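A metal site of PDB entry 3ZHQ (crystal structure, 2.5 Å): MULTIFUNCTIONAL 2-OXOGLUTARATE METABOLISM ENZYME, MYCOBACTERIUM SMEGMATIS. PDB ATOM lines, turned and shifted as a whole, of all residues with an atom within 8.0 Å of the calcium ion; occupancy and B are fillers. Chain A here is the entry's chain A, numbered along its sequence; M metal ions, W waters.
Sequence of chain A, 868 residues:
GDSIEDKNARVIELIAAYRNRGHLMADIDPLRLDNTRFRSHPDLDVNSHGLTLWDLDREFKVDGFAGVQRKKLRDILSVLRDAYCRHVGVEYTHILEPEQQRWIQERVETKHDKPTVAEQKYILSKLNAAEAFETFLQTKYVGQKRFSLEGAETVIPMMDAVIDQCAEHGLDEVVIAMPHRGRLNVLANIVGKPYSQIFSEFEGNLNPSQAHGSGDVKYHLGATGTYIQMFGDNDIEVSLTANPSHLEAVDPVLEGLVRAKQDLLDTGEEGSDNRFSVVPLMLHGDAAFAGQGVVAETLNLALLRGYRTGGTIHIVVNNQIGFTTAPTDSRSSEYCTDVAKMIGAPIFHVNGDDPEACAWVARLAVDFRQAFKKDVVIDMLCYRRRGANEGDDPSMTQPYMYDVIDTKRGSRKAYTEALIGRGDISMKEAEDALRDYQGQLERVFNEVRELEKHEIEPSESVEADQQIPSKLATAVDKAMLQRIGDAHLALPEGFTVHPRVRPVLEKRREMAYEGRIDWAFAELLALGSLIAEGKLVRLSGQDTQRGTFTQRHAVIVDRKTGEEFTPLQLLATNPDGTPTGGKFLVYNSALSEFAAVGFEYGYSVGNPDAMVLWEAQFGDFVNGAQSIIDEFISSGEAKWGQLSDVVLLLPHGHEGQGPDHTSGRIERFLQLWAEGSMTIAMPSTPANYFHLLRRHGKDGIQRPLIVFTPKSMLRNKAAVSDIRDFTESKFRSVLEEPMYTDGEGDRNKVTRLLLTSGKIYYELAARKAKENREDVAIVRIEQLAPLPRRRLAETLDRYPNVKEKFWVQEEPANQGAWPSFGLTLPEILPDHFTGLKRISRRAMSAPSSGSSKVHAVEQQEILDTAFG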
ATOM      1  N   LYS A 535     -18.370 -23.587  -1.931  1.00  0.00           N
ATOM      2  CA  LYS A 535     -18.528 -24.092  -3.293  1.00  0.00           C
ATOM      3  C   LYS A 535     -18.629 -25.616  -3.376  1.00  0.00           C
ATOM      4  O   LYS A 535     -17.965 -26.326  -2.612  1.00  0.00           O
ATOM      5  CB  LYS A 535     -17.364 -23.629  -4.186  1.00  0.00           C
ATOM      6  CG  LYS A 535     -17.755 -23.505  -5.657  1.00  0.00           C
ATOM      7  CD  LYS A 535     -16.675 -22.892  -6.461  1.00  0.00           C
ATOM      8  CE  LYS A 535     -17.128 -22.665  -7.880  1.00  0.00           C
ATOM      9  NZ  LYS A 535     -18.175 -21.611  -7.978  1.00  0.00           N
ATOM     10  N   PRO A 608     -24.076 -24.114 -12.770  1.00  0.00           N
ATOM     11  CA  PRO A 608     -23.031 -23.120 -13.070  1.00  0.00           C
ATOM     12  C   PRO A 608     -22.198 -22.671 -11.857  1.00  0.00           C
ATOM     13  O   PRO A 608     -21.134 -22.114 -12.079  1.00  0.00           O
ATOM     14  CB  PRO A 608     -23.829 -21.923 -13.628  1.00  0.00           C
ATOM     15  CG  PRO A 608     -25.147 -22.467 -13.994  1.00  0.00           C
ATOM     16  CD  PRO A 608     -25.418 -23.549 -13.006  1.00  0.00           C
ATOM     17  N   ALA A 610     -20.902 -24.666  -9.559  1.00  0.00           N
ATOM     18  CA  ALA A 610     -20.065 -25.787  -9.183  1.00  0.00           C
ATOM     19  C   ALA A 610     -18.697 -25.695  -9.844  1.00  0.00           C
ATOM     20  O   ALA A 610     -18.561 -25.165 -10.954  1.00  0.00           O
ATOM     21  CB  ALA A 610     -20.735 -27.104  -9.590  1.00  0.00           C
ATOM     22  N   MET A 611     -17.677 -26.223  -9.152  1.00  0.00           N
ATOM     23  CA  MET A 611     -16.307 -26.336  -9.646  1.00  0.00           C
ATOM     24  C   MET A 611     -16.266 -27.746 -10.207  1.00  0.00           C
ATOM     25  O   MET A 611     -16.383 -28.691  -9.437  1.00  0.00           O
ATOM     26  CB  MET A 611     -15.286 -26.056  -8.523  1.00  0.00           C
ATOM     27  CG  MET A 611     -13.825 -26.127  -8.955  1.00  0.00           C
ATOM     28  SD  MET A 611     -13.271 -24.683  -9.882  1.00  0.00           S
ATOM     29  CE  MET A 611     -11.560 -25.110 -10.089  1.00  0.00           C
ATOM     30  N   SER A 644     -20.500 -23.104 -20.035  1.00  0.00           N
ATOM     31  CA  SER A 644     -19.909 -24.183 -19.239  1.00  0.00           C
ATOM     32  C   SER A 644     -18.623 -23.691 -18.619  1.00  0.00           C
ATOM     33  O   SER A 644     -17.883 -22.952 -19.249  1.00  0.00           O
ATOM     34  CB  SER A 644     -19.663 -25.406 -20.097  1.00  0.00           C
ATOM     35  OG  SER A 644     -19.056 -26.461 -19.374  1.00  0.00           O
ATOM     36  N   ASP A 645     -18.358 -24.084 -17.377  1.00  0.00           N
ATOM     37  CA  ASP A 645     -17.161 -23.684 -16.647  1.00  0.00           C
ATOM     38  C   ASP A 645     -16.314 -24.926 -16.340  1.00  0.00           C
ATOM     39  O   ASP A 645     -15.522 -24.925 -15.414  1.00  0.00           O
ATOM     40  CB  ASP A 645     -17.580 -22.969 -15.340  1.00  0.00           C
ATOM     41  CG  ASP A 645     -16.594 -21.964 -14.815  1.00  0.00           C
ATOM     42  OD1 ASP A 645     -16.015 -21.216 -15.633  1.00  0.00           O
ATOM     43  OD2 ASP A 645     -16.444 -21.867 -13.576  1.00  0.00           O
ATOM     44  N   VAL A 646     -16.478 -25.979 -17.165  1.00  0.00           N
ATOM     45  CA  VAL A 646     -15.796 -27.263 -17.005  1.00  0.00           C
ATOM     46  C   VAL A 646     -14.273 -27.074 -17.159  1.00  0.00           C
ATOM     47  O   VAL A 646     -13.819 -26.322 -18.031  1.00  0.00           O
ATOM     48  CB  VAL A 646     -16.366 -28.368 -17.968  1.00  0.00           C
ATOM     49  CG1 VAL A 646     -16.038 -28.112 -19.443  1.00  0.00           C
ATOM     50  CG2 VAL A 646     -15.920 -29.751 -17.547  1.00  0.00           C
ATOM     51  N   VAL A 647     -13.517 -27.763 -16.287  1.00  0.00           N
ATOM     52  CA  VAL A 647     -12.062 -27.814 -16.295  1.00  0.00           C
ATOM     53  C   VAL A 647     -11.629 -29.173 -16.843  1.00  0.00           C
ATOM     54  O   VAL A 647     -12.127 -30.198 -16.381  1.00  0.00           O
ATOM     55  CB  VAL A 647     -11.421 -27.558 -14.908  1.00  0.00           C
ATOM     56  CG1 VAL A 647      -9.894 -27.482 -14.984  1.00  0.00           C
ATOM     57  CG2 VAL A 647     -11.987 -26.303 -14.257  1.00  0.00           C
ATOM     58  N   THR A 679     -10.106 -20.830 -21.627  1.00  0.00           N
ATOM     59  CA  THR A 679      -8.841 -20.412 -21.032  1.00  0.00           C
ATOM     60  C   THR A 679      -7.923 -21.640 -21.165  1.00  0.00           C
ATOM     61  O   THR A 679      -8.353 -22.737 -20.856  1.00  0.00           O
ATOM     62  CB  THR A 679      -9.018 -19.898 -19.584  1.00  0.00           C
ATOM     63  OG1 THR A 679      -9.929 -18.793 -19.600  1.00  0.00           O
ATOM     64  CG2 THR A 679      -7.694 -19.426 -18.950  1.00  0.00           C
ATOM     65  N   LEU A 692      -4.857 -20.278 -10.399  1.00  0.00           N
ATOM     66  CA  LEU A 692      -5.571 -20.531 -11.653  1.00  0.00           C
ATOM     67  C   LEU A 692      -6.939 -21.178 -11.341  1.00  0.00           C
ATOM     68  O   LEU A 692      -7.962 -20.677 -11.821  1.00  0.00           O
ATOM     69  CB  LEU A 692      -4.712 -21.434 -12.573  1.00  0.00           C
ATOM     70  CG  LEU A 692      -5.306 -21.884 -13.922  1.00  0.00           C
ATOM     71  CD1 LEU A 692      -5.181 -20.793 -14.973  1.00  0.00           C
ATOM     72  CD2 LEU A 692      -4.661 -23.164 -14.390  1.00  0.00           C
ATOM     73  N   LEU A 693      -6.966 -22.230 -10.498  1.00  0.00           N
ATOM     74  CA  LEU A 693      -8.172 -22.935 -10.059  1.00  0.00           C
ATOM     75  C   LEU A 693      -9.092 -22.036  -9.212  1.00  0.00           C
ATOM     76  O   LEU A 693     -10.314 -22.004  -9.439  1.00  0.00           O
ATOM     77  CB  LEU A 693      -7.836 -24.216  -9.272  1.00  0.00           C
ATOM     78  CG  LEU A 693      -7.094 -25.344 -10.025  1.00  0.00           C
ATOM     79  CD1 LEU A 693      -6.861 -26.527  -9.126  1.00  0.00           C
ATOM     80  CD2 LEU A 693      -7.860 -25.760 -11.297  1.00  0.00           C
ATOM     81  N   ARG A 694      -8.516 -21.279  -8.278  1.00  0.00           N
ATOM     82  CA  ARG A 694      -9.328 -20.383  -7.457  1.00  0.00           C
ATOM     83  C   ARG A 694      -9.910 -19.201  -8.304  1.00  0.00           C
ATOM     84  O   ARG A 694     -11.070 -18.831  -8.099  1.00  0.00           O
ATOM     85  CB  ARG A 694      -8.526 -19.875  -6.250  1.00  0.00           C
ATOM     86  CG  ARG A 694      -8.557 -20.911  -5.149  1.00  0.00           C
ATOM     87  CD  ARG A 694      -7.948 -20.440  -3.859  1.00  0.00           C
ATOM     88  NE  ARG A 694      -8.517 -19.197  -3.334  1.00  0.00           N
ATOM     89  CZ  ARG A 694      -9.676 -19.105  -2.687  1.00  0.00           C
ATOM     90  NH1 ARG A 694     -10.445 -20.169  -2.527  1.00  0.00           N
ATOM     91  NH2 ARG A 694     -10.088 -17.928  -2.225  1.00  0.00           N
ATOM     92  N   ARG A 695      -9.145 -18.659  -9.277  1.00  0.00           N
ATOM     93  CA  ARG A 695      -9.646 -17.586 -10.167  1.00  0.00           C
ATOM     94  C   ARG A 695     -10.793 -18.142 -11.026  1.00  0.00           C
ATOM     95  O   ARG A 695     -11.845 -17.521 -11.092  1.00  0.00           O
ATOM     96  CB  ARG A 695      -8.515 -16.988 -11.035  1.00  0.00           C
ATOM     97  CG  ARG A 695      -8.974 -15.918 -12.030  1.00  0.00           C
ATOM     98  CD  ARG A 695      -7.864 -15.487 -12.972  1.00  0.00           C
ATOM     99  NE  ARG A 695      -7.546 -16.490 -13.986  1.00  0.00           N
ATOM    100  CZ  ARG A 695      -6.779 -16.270 -15.056  1.00  0.00           C
ATOM    101  NH1 ARG A 695      -6.262 -15.067 -15.261  1.00  0.00           N
ATOM    102  NH2 ARG A 695      -6.527 -17.234 -15.916  1.00  0.00           N
ATOM    103  N   HIS A 696     -10.609 -19.342 -11.616  1.00  0.00           N
ATOM    104  CA  HIS A 696     -11.591 -20.047 -12.455  1.00  0.00           C
ATOM    105  C   HIS A 696     -12.924 -20.276 -11.725  1.00  0.00           C
ATOM    106  O   HIS A 696     -13.980 -20.133 -12.341  1.00  0.00           O
ATOM    107  CB  HIS A 696     -11.049 -21.385 -12.952  1.00  0.00           C
ATOM    108  CG  HIS A 696     -12.031 -22.129 -13.805  1.00  0.00           C
ATOM    109  ND1 HIS A 696     -12.261 -21.758 -15.114  1.00  0.00           N
ATOM    110  CD2 HIS A 696     -12.869 -23.125 -13.479  1.00  0.00           C
ATOM    111  CE1 HIS A 696     -13.191 -22.595 -15.554  1.00  0.00           C
ATOM    112  NE2 HIS A 696     -13.599 -23.426 -14.600  1.00  0.00           N
ATOM    113  N   GLY A 697     -12.871 -20.644 -10.469  1.00  0.00           N
ATOM    114  CA  GLY A 697     -14.065 -20.920  -9.684  1.00  0.00           C
ATOM    115  C   GLY A 697     -14.698 -19.712  -9.049  1.00  0.00           C
ATOM    116  O   GLY A 697     -15.848 -19.796  -8.641  1.00  0.00           O
ATOM    117  N   LYS A 698     -13.980 -18.581  -8.960  1.00  0.00           N
ATOM    118  CA  LYS A 698     -14.515 -17.384  -8.303  1.00  0.00           C
ATOM    119  C   LYS A 698     -14.771 -16.177  -9.243  1.00  0.00           C
ATOM    120  O   LYS A 698     -15.429 -15.234  -8.796  1.00  0.00           O
ATOM    121  CB  LYS A 698     -13.565 -16.921  -7.199  1.00  0.00           C
ATOM    122  CG  LYS A 698     -13.353 -17.916  -6.059  1.00  0.00           C
ATOM    123  CD  LYS A 698     -12.186 -17.510  -5.150  1.00  0.00           C
ATOM    124  CE  LYS A 698     -12.524 -16.371  -4.217  1.00  0.00           C
ATOM    125  NZ  LYS A 698     -13.671 -16.709  -3.333  1.00  0.00           N
ATOM    126  N   ASP A 699     -14.282 -16.218 -10.503  1.00  0.00           N
ATOM    127  CA  ASP A 699     -14.360 -15.103 -11.452  1.00  0.00           C
ATOM    128  C   ASP A 699     -15.780 -14.744 -11.906  1.00  0.00           C
ATOM    129  O   ASP A 699     -15.946 -13.709 -12.576  1.00  0.00           O
ATOM    130  CB  ASP A 699     -13.458 -15.350 -12.679  1.00  0.00           C
ATOM    131  CG  ASP A 699     -13.754 -16.573 -13.524  1.00  0.00           C
ATOM    132  OD1 ASP A 699     -14.807 -17.218 -13.290  1.00  0.00           O
ATOM    133  OD2 ASP A 699     -12.948 -16.879 -14.417  1.00  0.00           O
ATOM    134  N   GLY A 700     -16.774 -15.578 -11.575  1.00  0.00           N
ATOM    135  CA  GLY A 700     -18.172 -15.347 -11.945  1.00  0.00           C
ATOM    136  C   GLY A 700     -18.447 -15.375 -13.437  1.00  0.00           C
ATOM    137  O   GLY A 700     -19.456 -14.831 -13.885  1.00  0.00           O
ATOM    138  N   ILE A 701     -17.550 -16.004 -14.215  1.00  0.00           N
ATOM    139  CA  ILE A 701     -17.607 -16.163 -15.669  1.00  0.00           C
ATOM    140  C   ILE A 701     -17.702 -17.641 -15.960  1.00  0.00           C
ATOM    141  O   ILE A 701     -16.956 -18.429 -15.378  1.00  0.00           O
ATOM    142  CB  ILE A 701     -16.344 -15.485 -16.304  1.00  0.00           C
ATOM    143  CG1 ILE A 701     -16.523 -13.954 -16.349  1.00  0.00           C
ATOM    144  CG2 ILE A 701     -15.999 -16.050 -17.711  1.00  0.00           C
ATOM    145  CD1 ILE A 701     -15.189 -13.126 -16.328  1.00  0.00           C
ATOM    146  N   GLN A 702     -18.615 -18.035 -16.850  1.00  0.00           N
ATOM    147  CA  GLN A 702     -18.761 -19.432 -17.230  1.00  0.00           C
ATOM    148  C   GLN A 702     -17.994 -19.648 -18.536  1.00  0.00           C
ATOM    149  O   GLN A 702     -18.456 -19.258 -19.610  1.00  0.00           O
ATOM    150  CB  GLN A 702     -20.243 -19.852 -17.324  1.00  0.00           C
ATOM    151  CG  GLN A 702     -21.038 -19.663 -16.019  1.00  0.00           C
ATOM    152  CD  GLN A 702     -20.512 -20.540 -14.911  1.00  0.00           C
ATOM    153  OE1 GLN A 702     -20.564 -21.772 -14.993  1.00  0.00           O
ATOM    154  NE2 GLN A 702     -19.955 -19.928 -13.879  1.00  0.00           N
ATOM    155  N   ARG A 703     -16.777 -20.185 -18.415  1.00  0.00           N
ATOM    156  CA  ARG A 703     -15.887 -20.431 -19.549  1.00  0.00           C
ATOM    157  C   ARG A 703     -15.019 -21.648 -19.278  1.00  0.00           C
ATOM    158  O   ARG A 703     -14.397 -21.700 -18.212  1.00  0.00           O
ATOM    159  CB  ARG A 703     -15.026 -19.182 -19.813  1.00  0.00           C
ATOM    160  CG  ARG A 703     -14.149 -19.263 -21.066  1.00  0.00           C
ATOM    161  CD  ARG A 703     -13.515 -17.928 -21.348  1.00  0.00           C
ATOM    162  NE  ARG A 703     -14.532 -16.929 -21.643  1.00  0.00           N
ATOM    163  CZ  ARG A 703     -14.428 -15.634 -21.376  1.00  0.00           C
ATOM    164  NH1 ARG A 703     -13.323 -15.166 -20.829  1.00  0.00           N
ATOM    165  NH2 ARG A 703     -15.412 -14.805 -21.681  1.00  0.00           N
ATOM    166  N   PRO A 704     -14.901 -22.621 -20.218  1.00  0.00           N
ATOM    167  CA  PRO A 704     -14.046 -23.795 -19.947  1.00  0.00           C
ATOM    168  C   PRO A 704     -12.579 -23.424 -19.763  1.00  0.00           C
ATOM    169  O   PRO A 704     -12.094 -22.468 -20.364  1.00  0.00           O
ATOM    170  CB  PRO A 704     -14.252 -24.663 -21.187  1.00  0.00           C
ATOM    171  CG  PRO A 704     -15.569 -24.187 -21.780  1.00  0.00           C
ATOM    172  CD  PRO A 704     -15.548 -22.734 -21.546  1.00  0.00           C
ATOM    173  N   LEU A 705     -11.886 -24.174 -18.888  1.00  0.00           N
ATOM    174  CA  LEU A 705     -10.473 -24.056 -18.603  1.00  0.00           C
ATOM    175  C   LEU A 705      -9.769 -25.351 -19.002  1.00  0.00           C
ATOM    176  O   LEU A 705     -10.174 -26.435 -18.587  1.00  0.00           O
ATOM    177  CB  LEU A 705     -10.255 -23.726 -17.111  1.00  0.00           C
ATOM    178  CG  LEU A 705      -8.789 -23.773 -16.551  1.00  0.00           C
ATOM    179  CD1 LEU A 705      -7.872 -22.725 -17.214  1.00  0.00           C
ATOM    180  CD2 LEU A 705      -8.780 -23.587 -15.045  1.00  0.00           C
HETATM  181 CA    CA M   1     -15.448 -19.520 -14.017  1.00  0.00          CA
HETATM  182  O   HOH W   1     -17.409 -19.207 -12.058  1.00  0.00           O
HETATM  183  O   HOH W   2     -13.689 -18.938 -15.720  1.00  0.00           O
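The calcium ion is bound by O of Ile 701 (2.3 Å), O of His 696 (2.3 Å), OD1 of Asp 645 (2.4 Å), OD1 of Asp 699 (2.5 Å), water W2 (2.5 Å), OD2 of Asp 645 (2.6 Å) and water W1 (2.8 Å).
The backbone NH of Arg 703 lies close to the side-chain carboxylate of Asp 645 (3.1 Å).
Within 4 Å of the calcium ion: Asp 645, His 696, Asp 699 and Ile 701.
Water W2 bridges OD2 of Asp 699 and ND1 of His 696.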
